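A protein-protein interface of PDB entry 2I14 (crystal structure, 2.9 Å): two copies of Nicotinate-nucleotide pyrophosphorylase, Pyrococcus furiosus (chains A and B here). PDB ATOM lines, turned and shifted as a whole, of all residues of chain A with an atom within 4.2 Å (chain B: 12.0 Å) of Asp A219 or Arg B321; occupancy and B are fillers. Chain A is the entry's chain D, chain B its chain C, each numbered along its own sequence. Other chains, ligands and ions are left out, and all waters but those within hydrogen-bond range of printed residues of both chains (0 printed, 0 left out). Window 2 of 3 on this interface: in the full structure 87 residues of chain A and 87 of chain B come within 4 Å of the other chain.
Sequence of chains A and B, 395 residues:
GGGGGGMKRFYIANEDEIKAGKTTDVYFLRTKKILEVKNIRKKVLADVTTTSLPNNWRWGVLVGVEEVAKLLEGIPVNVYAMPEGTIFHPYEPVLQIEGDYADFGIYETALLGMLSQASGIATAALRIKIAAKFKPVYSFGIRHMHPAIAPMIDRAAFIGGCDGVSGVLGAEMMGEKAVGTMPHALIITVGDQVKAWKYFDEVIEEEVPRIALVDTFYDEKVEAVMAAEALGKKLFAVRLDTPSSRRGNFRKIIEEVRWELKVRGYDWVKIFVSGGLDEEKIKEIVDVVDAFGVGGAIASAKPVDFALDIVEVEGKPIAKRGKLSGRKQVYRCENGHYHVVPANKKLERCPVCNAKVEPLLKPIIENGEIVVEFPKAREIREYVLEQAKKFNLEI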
ATOM      1  N   ASP A 215       5.565  -8.927  29.807  1.00  0.00           N
ATOM      2  CA  ASP A 215       5.104  -8.882  28.415  1.00  0.00           C
ATOM      3  C   ASP A 215       4.332  -7.615  28.042  1.00  0.00           C
ATOM      4  O   ASP A 215       3.202  -7.438  28.492  1.00  0.00           O
ATOM      5  CB  ASP A 215       4.205 -10.093  28.141  1.00  0.00           C
ATOM      6  CG  ASP A 215       3.536 -10.031  26.778  1.00  0.00           C
ATOM      7  OD1 ASP A 215       2.869  -9.014  26.488  1.00  0.00           O
ATOM      8  OD2 ASP A 215       3.669 -11.001  25.994  1.00  0.00           O
ATOM      9  N   THR A 216       4.918  -6.753  27.212  1.00  0.00           N
ATOM     10  CA  THR A 216       4.249  -5.517  26.776  1.00  0.00           C
ATOM     11  C   THR A 216       4.655  -5.166  25.346  1.00  0.00           C
ATOM     12  O   THR A 216       3.804  -5.040  24.469  1.00  0.00           O
ATOM     13  CB  THR A 216       4.585  -4.294  27.686  1.00  0.00           C
ATOM     14  OG1 THR A 216       4.286  -4.596  29.058  1.00  0.00           O
ATOM     15  CG2 THR A 216       3.756  -3.077  27.262  1.00  0.00           C
ATOM     16  N   TYR A 218       8.415  -6.026  24.402  1.00  0.00           N
ATOM     17  CA  TYR A 218       9.481  -7.003  24.241  1.00  0.00           C
ATOM     18  C   TYR A 218       8.951  -8.369  24.669  1.00  0.00           C
ATOM     19  O   TYR A 218       7.856  -8.460  25.216  1.00  0.00           O
ATOM     20  CB  TYR A 218      10.670  -6.616  25.126  1.00  0.00           C
ATOM     21  CG  TYR A 218      11.229  -5.219  24.897  1.00  0.00           C
ATOM     22  CD1 TYR A 218      10.391  -4.106  24.832  1.00  0.00           C
ATOM     23  CD2 TYR A 218      12.609  -5.004  24.800  1.00  0.00           C
ATOM     24  CE1 TYR A 218      10.910  -2.814  24.678  1.00  0.00           C
ATOM     25  CE2 TYR A 218      13.134  -3.716  24.651  1.00  0.00           C
ATOM     26  CZ  TYR A 218      12.279  -2.627  24.591  1.00  0.00           C
ATOM     27  OH  TYR A 218      12.791  -1.357  24.454  1.00  0.00           O
ATOM     28  N   ASP A 219       9.719  -9.427  24.425  1.00  0.00           N
ATOM     29  CA  ASP A 219       9.302 -10.775  24.820  1.00  0.00           C
ATOM     30  C   ASP A 219       9.347 -10.901  26.350  1.00  0.00           C
ATOM     31  O   ASP A 219      10.078 -10.168  27.018  1.00  0.00           O
ATOM     32  CB  ASP A 219      10.227 -11.821  24.184  1.00  0.00           C
ATOM     33  CG  ASP A 219       9.698 -13.235  24.324  1.00  0.00           C
ATOM     34  OD1 ASP A 219       8.611 -13.523  23.775  1.00  0.00           O
ATOM     35  OD2 ASP A 219      10.368 -14.060  24.979  1.00  0.00           O
ATOM     36  N   GLU A 220       8.565 -11.819  26.910  1.00  0.00           N
ATOM     37  CA  GLU A 220       8.555 -11.994  28.358  1.00  0.00           C
ATOM     38  C   GLU A 220       9.971 -12.301  28.833  1.00  0.00           C
ATOM     39  O   GLU A 220      10.405 -11.832  29.890  1.00  0.00           O
ATOM     40  CB  GLU A 220       7.635 -13.146  28.772  1.00  0.00           C
ATOM     41  CG  GLU A 220       6.205 -13.060  28.271  1.00  0.00           C
ATOM     42  CD  GLU A 220       6.055 -13.552  26.846  1.00  0.00           C
ATOM     43  OE1 GLU A 220       4.918 -13.555  26.336  1.00  0.00           O
ATOM     44  OE2 GLU A 220       7.069 -13.944  26.234  1.00  0.00           O
ATOM     45  N   LYS A 221      10.688 -13.088  28.037  1.00  0.00           N
ATOM     46  CA  LYS A 221      12.051 -13.476  28.371  1.00  0.00           C
ATOM     47  C   LYS A 221      12.944 -12.258  28.572  1.00  0.00           C
ATOM     48  O   LYS A 221      13.705 -12.180  29.534  1.00  0.00           O
ATOM     49  CB  LYS A 221      12.633 -14.364  27.271  1.00  0.00           C
ATOM     50  CG  LYS A 221      13.996 -14.934  27.600  1.00  0.00           C
ATOM     51  CD  LYS A 221      14.352 -16.087  26.671  1.00  0.00           C
ATOM     52  CE  LYS A 221      15.047 -15.631  25.409  1.00  0.00           C
ATOM     53  NZ  LYS A 221      16.454 -15.279  25.710  1.00  0.00           N
ATOM     54  N   VAL A 222      12.844 -11.304  27.658  1.00  0.00           N
ATOM     55  CA  VAL A 222      13.658 -10.104  27.746  1.00  0.00           C
ATOM     56  C   VAL A 222      13.227  -9.204  28.899  1.00  0.00           C
ATOM     57  O   VAL A 222      14.028  -8.891  29.772  1.00  0.00           O
ATOM     58  CB  VAL A 222      13.604  -9.304  26.432  1.00  0.00           C
ATOM     59  CG1 VAL A 222      14.540  -8.113  26.519  1.00  0.00           C
ATOM     60  CG2 VAL A 222      13.975 -10.203  25.261  1.00  0.00           C
ATOM     61  N   GLU A 223      11.961  -8.793  28.905  1.00  0.00           N
ATOM     62  CA  GLU A 223      11.444  -7.915  29.953  1.00  0.00           C
ATOM     63  C   GLU A 223      11.485  -8.510  31.350  1.00  0.00           C
ATOM     64  O   GLU A 223      11.418  -7.778  32.340  1.00  0.00           O
ATOM     65  CB  GLU A 223      10.016  -7.493  29.633  1.00  0.00           C
ATOM     66  CG  GLU A 223       9.929  -6.538  28.467  1.00  0.00           C
ATOM     67  CD  GLU A 223       8.567  -5.887  28.353  1.00  0.00           C
ATOM     68  OE1 GLU A 223       8.119  -5.248  29.333  1.00  0.00           O
ATOM     69  OE2 GLU A 223       7.949  -6.011  27.275  1.00  0.00           O
ATOM     70  N   PRO A 243      -0.635 -13.039  25.434  1.00  0.00           N
ATOM     71  CA  PRO A 243      -1.872 -12.970  24.652  1.00  0.00           C
ATOM     72  C   PRO A 243      -2.057 -14.305  23.926  1.00  0.00           C
ATOM     73  O   PRO A 243      -1.081 -14.977  23.587  1.00  0.00           O
ATOM     74  CB  PRO A 243      -1.602 -11.820  23.686  1.00  0.00           C
ATOM     75  CG  PRO A 243      -0.699 -10.919  24.489  1.00  0.00           C
ATOM     76  CD  PRO A 243       0.255 -11.906  25.114  1.00  0.00           C
ATOM     77  N   ARG A 246      -0.153 -15.248  21.083  1.00  0.00           N
ATOM     78  CA  ARG A 246       1.247 -15.532  21.379  1.00  0.00           C
ATOM     79  C   ARG A 246       1.499 -16.801  22.203  1.00  0.00           C
ATOM     80  O   ARG A 246       2.616 -17.312  22.217  1.00  0.00           O
ATOM     81  CB  ARG A 246       1.878 -14.304  22.068  1.00  0.00           C
ATOM     82  CG  ARG A 246       1.748 -13.008  21.249  1.00  0.00           C
ATOM     83  CD  ARG A 246       2.461 -13.153  19.897  1.00  0.00           C
ATOM     84  NE  ARG A 246       2.042 -12.159  18.902  1.00  0.00           N
ATOM     85  CZ  ARG A 246       2.249 -10.848  19.004  1.00  0.00           C
ATOM     86  NH1 ARG A 246       2.875 -10.356  20.068  1.00  0.00           N
ATOM     87  NH2 ARG A 246       1.830 -10.028  18.040  1.00  0.00           N
ATOM     88  N   ASP B  47      -9.165   1.815  22.853  1.00  0.00           N
ATOM     89  CA  ASP B  47     -10.073   1.028  22.025  1.00  0.00           C
ATOM     90  C   ASP B  47     -10.741  -0.070  22.843  1.00  0.00           C
ATOM     91  O   ASP B  47     -10.162  -0.566  23.811  1.00  0.00           O
ATOM     92  CB  ASP B  47      -9.280   0.357  20.907  1.00  0.00           C
ATOM     93  CG  ASP B  47      -9.611   0.903  19.535  1.00  0.00           C
ATOM     94  OD1 ASP B  47     -10.288   1.952  19.465  1.00  0.00           O
ATOM     95  OD2 ASP B  47      -9.185   0.294  18.525  1.00  0.00           O
ATOM     96  N   THR B  49     -12.452  -3.764  22.185  1.00  0.00           N
ATOM     97  CA  THR B  49     -12.655  -4.837  21.208  1.00  0.00           C
ATOM     98  C   THR B  49     -12.593  -6.190  21.885  1.00  0.00           C
ATOM     99  O   THR B  49     -12.497  -6.273  23.104  1.00  0.00           O
ATOM    100  CB  THR B  49     -11.528  -4.864  20.137  1.00  0.00           C
ATOM    101  OG1 THR B  49     -10.296  -5.194  20.782  1.00  0.00           O
ATOM    102  CG2 THR B  49     -11.354  -3.513  19.451  1.00  0.00           C
ATOM    103  N   THR B  50     -12.661  -7.244  21.079  1.00  0.00           N
ATOM    104  CA  THR B  50     -12.543  -8.619  21.557  1.00  0.00           C
ATOM    105  C   THR B  50     -11.773  -9.294  20.466  1.00  0.00           C
ATOM    106  O   THR B  50     -11.896  -8.932  19.301  1.00  0.00           O
ATOM    107  CB  THR B  50     -13.880  -9.408  21.669  1.00  0.00           C
ATOM    108  OG1 THR B  50     -14.514  -9.495  20.388  1.00  0.00           O
ATOM    109  CG2 THR B  50     -14.815  -8.759  22.628  1.00  0.00           C
ATOM    110  N   THR B  51     -10.984 -10.285  20.841  1.00  0.00           N
ATOM    111  CA  THR B  51     -10.187 -11.029  19.879  1.00  0.00           C
ATOM    112  C   THR B  51     -10.974 -12.266  19.511  1.00  0.00           C
ATOM    113  O   THR B  51     -10.597 -13.017  18.630  1.00  0.00           O
ATOM    114  CB  THR B  51      -8.842 -11.450  20.491  1.00  0.00           C
ATOM    115  OG1 THR B  51      -9.079 -12.149  21.718  1.00  0.00           O
ATOM    116  CG2 THR B  51      -7.980 -10.239  20.766  1.00  0.00           C
ATOM    117  N   TYR B  91     -11.794  -7.680  16.708  1.00  0.00           N
ATOM    118  CA  TYR B  91     -10.848  -6.686  16.209  1.00  0.00           C
ATOM    119  C   TYR B  91     -11.447  -5.362  15.749  1.00  0.00           C
ATOM    120  O   TYR B  91     -10.724  -4.433  15.400  1.00  0.00           O
ATOM    121  CB  TYR B  91      -9.982  -7.297  15.110  1.00  0.00           C
ATOM    122  CG  TYR B  91      -9.153  -8.431  15.650  1.00  0.00           C
ATOM    123  CD1 TYR B  91      -9.690  -9.706  15.797  1.00  0.00           C
ATOM    124  CD2 TYR B  91      -7.858  -8.213  16.098  1.00  0.00           C
ATOM    125  CE1 TYR B  91      -8.955 -10.743  16.386  1.00  0.00           C
ATOM    126  CE2 TYR B  91      -7.112  -9.238  16.690  1.00  0.00           C
ATOM    127  CZ  TYR B  91      -7.669 -10.498  16.834  1.00  0.00           C
ATOM    128  OH  TYR B  91      -6.952 -11.493  17.454  1.00  0.00           O
ATOM    129  N   ASP B 305     -15.589 -11.299  25.707  1.00  0.00           N
ATOM    130  CA  ASP B 305     -14.299 -10.896  26.281  1.00  0.00           C
ATOM    131  C   ASP B 305     -13.887  -9.528  25.760  1.00  0.00           C
ATOM    132  O   ASP B 305     -12.960  -9.432  24.959  1.00  0.00           O
ATOM    133  CB  ASP B 305     -13.206 -11.941  25.953  1.00  0.00           C
ATOM    134  CG  ASP B 305     -12.113 -12.027  27.031  1.00  0.00           C
ATOM    135  OD1 ASP B 305     -11.031 -12.619  26.766  1.00  0.00           O
ATOM    136  OD2 ASP B 305     -12.337 -11.512  28.154  1.00  0.00           O
ATOM    137  N   ALA B 307     -12.171  -5.892  25.884  1.00  0.00           N
ATOM    138  CA  ALA B 307     -11.029  -5.304  26.568  1.00  0.00           C
ATOM    139  C   ALA B 307     -10.770  -3.865  26.128  1.00  0.00           C
ATOM    140  O   ALA B 307     -10.994  -3.515  24.973  1.00  0.00           O
ATOM    141  CB  ALA B 307      -9.798  -6.153  26.331  1.00  0.00           C
ATOM    142  N   LEU B 308     -10.306  -3.040  27.065  1.00  0.00           N
ATOM    143  CA  LEU B 308      -9.994  -1.639  26.793  1.00  0.00           C
ATOM    144  C   LEU B 308      -8.477  -1.498  26.658  1.00  0.00           C
ATOM    145  O   LEU B 308      -7.740  -1.707  27.625  1.00  0.00           O
ATOM    146  CB  LEU B 308     -10.509  -0.756  27.943  1.00  0.00           C
ATOM    147  CG  LEU B 308     -10.312   0.766  27.885  1.00  0.00           C
ATOM    148  CD1 LEU B 308      -8.850   1.158  28.113  1.00  0.00           C
ATOM    149  CD2 LEU B 308     -10.794   1.265  26.536  1.00  0.00           C
ATOM    150  N   ASP B 309      -8.012  -1.141  25.465  1.00  0.00           N
ATOM    151  CA  ASP B 309      -6.576  -0.994  25.229  1.00  0.00           C
ATOM    152  C   ASP B 309      -6.192   0.293  24.501  1.00  0.00           C
ATOM    153  O   ASP B 309      -6.718   0.590  23.427  1.00  0.00           O
ATOM    154  CB  ASP B 309      -6.034  -2.170  24.409  1.00  0.00           C
ATOM    155  CG  ASP B 309      -6.453  -3.510  24.956  1.00  0.00           C
ATOM    156  OD1 ASP B 309      -6.410  -3.696  26.189  1.00  0.00           O
ATOM    157  OD2 ASP B 309      -6.814  -4.392  24.146  1.00  0.00           O
ATOM    158  N   ILE B 310      -5.255   1.042  25.079  1.00  0.00           N
ATOM    159  CA  ILE B 310      -4.783   2.273  24.454  1.00  0.00           C
ATOM    160  C   ILE B 310      -4.045   1.936  23.158  1.00  0.00           C
ATOM    161  O   ILE B 310      -3.041   1.235  23.164  1.00  0.00           O
ATOM    162  CB  ILE B 310      -3.866   3.071  25.415  1.00  0.00           C
ATOM    163  CG1 ILE B 310      -3.047   2.115  26.267  1.00  0.00           C
ATOM    164  CG2 ILE B 310      -4.703   3.949  26.332  1.00  0.00           C
ATOM    165  CD1 ILE B 310      -2.404   2.789  27.455  1.00  0.00           C
ATOM    166  N   VAL B 311      -4.577   2.429  22.047  1.00  0.00           N
ATOM    167  CA  VAL B 311      -4.019   2.182  20.724  1.00  0.00           C
ATOM    168  C   VAL B 311      -3.304   3.408  20.165  1.00  0.00           C
ATOM    169  O   VAL B 311      -2.724   3.363  19.080  1.00  0.00           O
ATOM    170  CB  VAL B 311      -5.127   1.783  19.738  1.00  0.00           C
ATOM    171  CG1 VAL B 311      -5.905   0.615  20.290  1.00  0.00           C
ATOM    172  CG2 VAL B 311      -6.050   2.951  19.500  1.00  0.00           C
ATOM    173  N   GLU B 312      -3.362   4.507  20.911  1.00  0.00           N
ATOM    174  CA  GLU B 312      -2.722   5.746  20.497  1.00  0.00           C
ATOM    175  C   GLU B 312      -2.497   6.676  21.685  1.00  0.00           C
ATOM    176  O   GLU B 312      -3.401   6.897  22.494  1.00  0.00           O
ATOM    177  CB  GLU B 312      -3.578   6.450  19.442  1.00  0.00           C
ATOM    178  CG  GLU B 312      -2.791   7.423  18.575  1.00  0.00           C
ATOM    179  CD  GLU B 312      -3.625   8.041  17.466  1.00  0.00           C
ATOM    180  OE1 GLU B 312      -4.584   8.778  17.791  1.00  0.00           O
ATOM    181  OE2 GLU B 312      -3.317   7.787  16.277  1.00  0.00           O
ATOM    182  N   PRO B 317       0.689   6.336  17.269  1.00  0.00           N
ATOM    183  CA  PRO B 317       0.179   4.963  17.194  1.00  0.00           C
ATOM    184  C   PRO B 317       0.990   3.971  18.027  1.00  0.00           C
ATOM    185  O   PRO B 317       2.124   3.641  17.676  1.00  0.00           O
ATOM    186  CB  PRO B 317       0.269   4.641  15.705  1.00  0.00           C
ATOM    187  CG  PRO B 317       0.147   5.968  15.062  1.00  0.00           C
ATOM    188  CD  PRO B 317       1.033   6.819  15.924  1.00  0.00           C
ATOM    189  N   ILE B 318       0.399   3.490  19.121  1.00  0.00           N
ATOM    190  CA  ILE B 318       1.066   2.526  19.991  1.00  0.00           C
ATOM    191  C   ILE B 318       0.078   1.697  20.801  1.00  0.00           C
ATOM    192  O   ILE B 318      -0.815   2.244  21.453  1.00  0.00           O
ATOM    193  CB  ILE B 318       2.062   3.240  20.948  1.00  0.00           C
ATOM    194  CG1 ILE B 318       3.380   3.482  20.208  1.00  0.00           C
ATOM    195  CG2 ILE B 318       2.298   2.419  22.206  1.00  0.00           C
ATOM    196  CD1 ILE B 318       4.444   4.178  21.027  1.00  0.00           C
ATOM    197  N   ALA B 319       0.253   0.376  20.745  1.00  0.00           N
ATOM    198  CA  ALA B 319      -0.580  -0.586  21.472  1.00  0.00           C
ATOM    199  C   ALA B 319       0.282  -1.800  21.823  1.00  0.00           C
ATOM    200  O   ALA B 319       1.221  -2.121  21.096  1.00  0.00           O
ATOM    201  CB  ALA B 319      -1.755  -1.016  20.610  1.00  0.00           C
ATOM    202  N   LYS B 320      -0.028  -2.479  22.923  1.00  0.00           N
ATOM    203  CA  LYS B 320       0.754  -3.657  23.323  1.00  0.00           C
ATOM    204  C   LYS B 320       0.604  -4.857  22.372  1.00  0.00           C
ATOM    205  O   LYS B 320      -0.139  -4.788  21.395  1.00  0.00           O
ATOM    206  CB  LYS B 320       0.396  -4.057  24.762  1.00  0.00           C
ATOM    207  CG  LYS B 320      -1.072  -3.873  25.112  1.00  0.00           C
ATOM    208  CD  LYS B 320      -1.932  -4.910  24.428  1.00  0.00           C
ATOM    209  CE  LYS B 320      -1.679  -6.269  25.033  1.00  0.00           C
ATOM    210  NZ  LYS B 320      -2.007  -6.248  26.484  1.00  0.00           N
ATOM    211  N   ARG B 321       1.320  -5.946  22.665  1.00  0.00           N
ATOM    212  CA  ARG B 321       1.307  -7.167  21.834  1.00  0.00           C
ATOM    213  C   ARG B 321      -0.074  -7.773  21.602  1.00  0.00           C
ATOM    214  O   ARG B 321      -0.888  -7.868  22.521  1.00  0.00           O
ATOM    215  CB  ARG B 321       2.196  -8.255  22.449  1.00  0.00           C
ATOM    216  CG  ARG B 321       3.662  -7.903  22.604  1.00  0.00           C
ATOM    217  CD  ARG B 321       4.394  -9.014  23.351  1.00  0.00           C
ATOM    218  NE  ARG B 321       4.583 -10.208  22.530  1.00  0.00           N
ATOM    219  CZ  ARG B 321       5.037 -11.374  22.986  1.00  0.00           C
ATOM    220  NH1 ARG B 321       5.344 -11.516  24.266  1.00  0.00           N
ATOM    221  NH2 ARG B 321       5.207 -12.394  22.155  1.00  0.00           N
ATOM    222  N   GLY B 322      -0.318  -8.205  20.371  1.00  0.00           N
ATOM    223  CA  GLY B 322      -1.597  -8.803  20.041  1.00  0.00           C
ATOM    224  C   GLY B 322      -2.741  -7.811  19.950  1.00  0.00           C
ATOM    225  O   GLY B 322      -3.890  -8.210  19.824  1.00  0.00           O
ATOM    226  N   LYS B 323      -2.429  -6.522  20.020  1.00  0.00           N
ATOM    227  CA  LYS B 323      -3.444  -5.480  19.928  1.00  0.00           C
ATOM    228  C   LYS B 323      -3.143  -4.594  18.707  1.00  0.00           C
ATOM    229  O   LYS B 323      -1.979  -4.323  18.388  1.00  0.00           O
ATOM    230  CB  LYS B 323      -3.455  -4.630  21.201  1.00  0.00           C
ATOM    231  CG  LYS B 323      -4.844  -4.178  21.634  1.00  0.00           C
ATOM    232  CD  LYS B 323      -5.641  -3.504  20.503  1.00  0.00           C
ATOM    233  CE  LYS B 323      -7.079  -3.174  20.939  1.00  0.00           C
ATOM    234  NZ  LYS B 323      -7.926  -2.666  19.829  1.00  0.00           N
ATOM    235  N   LEU B 324      -4.196  -4.160  18.020  1.00  0.00           N
ATOM    236  CA  LEU B 324      -4.047  -3.314  16.848  1.00  0.00           C
ATOM    237  C   LEU B 324      -3.766  -1.900  17.292  1.00  0.00           C
ATOM    238  O   LEU B 324      -4.302  -1.435  18.293  1.00  0.00           O
ATOM    239  CB  LEU B 324      -5.310  -3.371  16.006  1.00  0.00           C
ATOM    240  CG  LEU B 324      -5.582  -4.778  15.460  1.00  0.00           C
ATOM    241  CD1 LEU B 324      -6.904  -4.774  14.706  1.00  0.00           C
ATOM    242  CD2 LEU B 324      -4.437  -5.233  14.555  1.00  0.00           C
ATOM    243  N   SER B 325      -2.928  -1.212  16.531  1.00  0.00           N
ATOM    244  CA  SER B 325      -2.524   0.141  16.884  1.00  0.00           C
ATOM    245  C   SER B 325      -3.163   1.248  16.053  1.00  0.00           C
ATOM    246  O   SER B 325      -3.501   1.049  14.887  1.00  0.00           O
ATOM    247  CB  SER B 325      -1.000   0.240  16.767  1.00  0.00           C
ATOM    248  OG  SER B 325      -0.458   1.170  17.686  1.00  0.00           O
ATOM    249  N   GLY B 326      -3.330   2.416  16.665  1.00  0.00           N
ATOM    250  CA  GLY B 326      -3.878   3.553  15.946  1.00  0.00           C
ATOM    251  C   GLY B 326      -5.354   3.855  16.088  1.00  0.00           C
ATOM    252  O   GLY B 326      -6.136   3.003  16.504  1.00  0.00           O
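Of the 22 printed residues of chain B, 3 touch a printed residue of chain A.
Printed residues of chain B that touch a printed residue of chain A: Lys B320, Arg B321 and Gly B322.
Of the 10 printed residues of chain A, 7 touch a printed residue of chain B.
Hydrophobic or aromatic side chains of chain A that line the printed part of chain B: Pro A243.
Among the printed residues, 9 pairs touch across the chains.
Among the printed residues, Asp or Glu carboxylates within 4 Å of a Lys or Arg side-chain nitrogen of the other chain: Asp A215 with Arg B321, Asp A219 with Arg B321 and Glu A220 with Arg B321.
Among the printed residues, pairs that only touch across the chains: Thr A216 with Lys B320 (3.5 Å), Tyr A218 with Arg B321 (3.97 Å), Pro A243 with Arg B321 (3.6 Å) and Arg A246 with Gly B322 (3.7 Å).
No position is printed for both chains.
Of the 9 pairs that touch across the chains among the printed residues, none has its exchanged pair printed and touching as well.
N of Thr A216 lies within hydrogen-bond range of OE2 of Glu A223 (3.1 Å).
The side-chain carboxylate (OE2) of Glu A223 sits at hydrogen-bond distance from the backbone NH (N) of Tyr A218 (2.9 Å).
OD2 of Asp A219 sits close to N of Lys A221, 3.2 Å away.
NH1 of Arg B321 is in salt-bridge range of OD2 of Asp A215, 2.5 Å away.
The backbone carbonyl oxygen of Thr A216 lies within hydrogen-bond range of the backbone NH of Arg B321 (3.2 Å).
The guanidinium group of Arg B321 lies within salt-bridge range of the side-chain carboxylate of Asp A219.
The guanidinium group (NH1) of Arg B321 lies within salt-bridge range of the side-chain carboxylate (OE1) of Glu A220, 2.9 Å away.
The guanidinium group of Arg B321 sits close to the guanidinium group of Arg A246, 3.0 Å away.
Arg B321 touches just these residues of chain A: Asp A215, Thr A216, Tyr A218, Asp A219, Glu A220, Pro A243 and Arg A246.
Asp A215 touches one residue of chain B.
Thr A216 touches just these residues of chain B: Lys B320 (3.5 Å) and Arg B321 (3.2 Å).
Glu A220 touches one residue of chain B.
Val A222 touches none of the printed residues of chain B.
No residue of chain B comes within 4 Å of Glu A223.
Of chain B, only Arg B321 (3.6 Å) comes within 4 Å of Pro A243.
Printed residues of chain A within 4 Å of Gly B322: Arg A246.
Printed residues of chain A within 4 Å of Lys B320: Thr A216 (3.5 Å).
Printed residues of chain B within 4 Å of Tyr A218: Arg B321 (3.97 Å).
Lys B323 touches none of the printed residues of chain A.
The nearest residue of chain B that does not touch Asp A219 is Lys B320 (10.4 Å).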
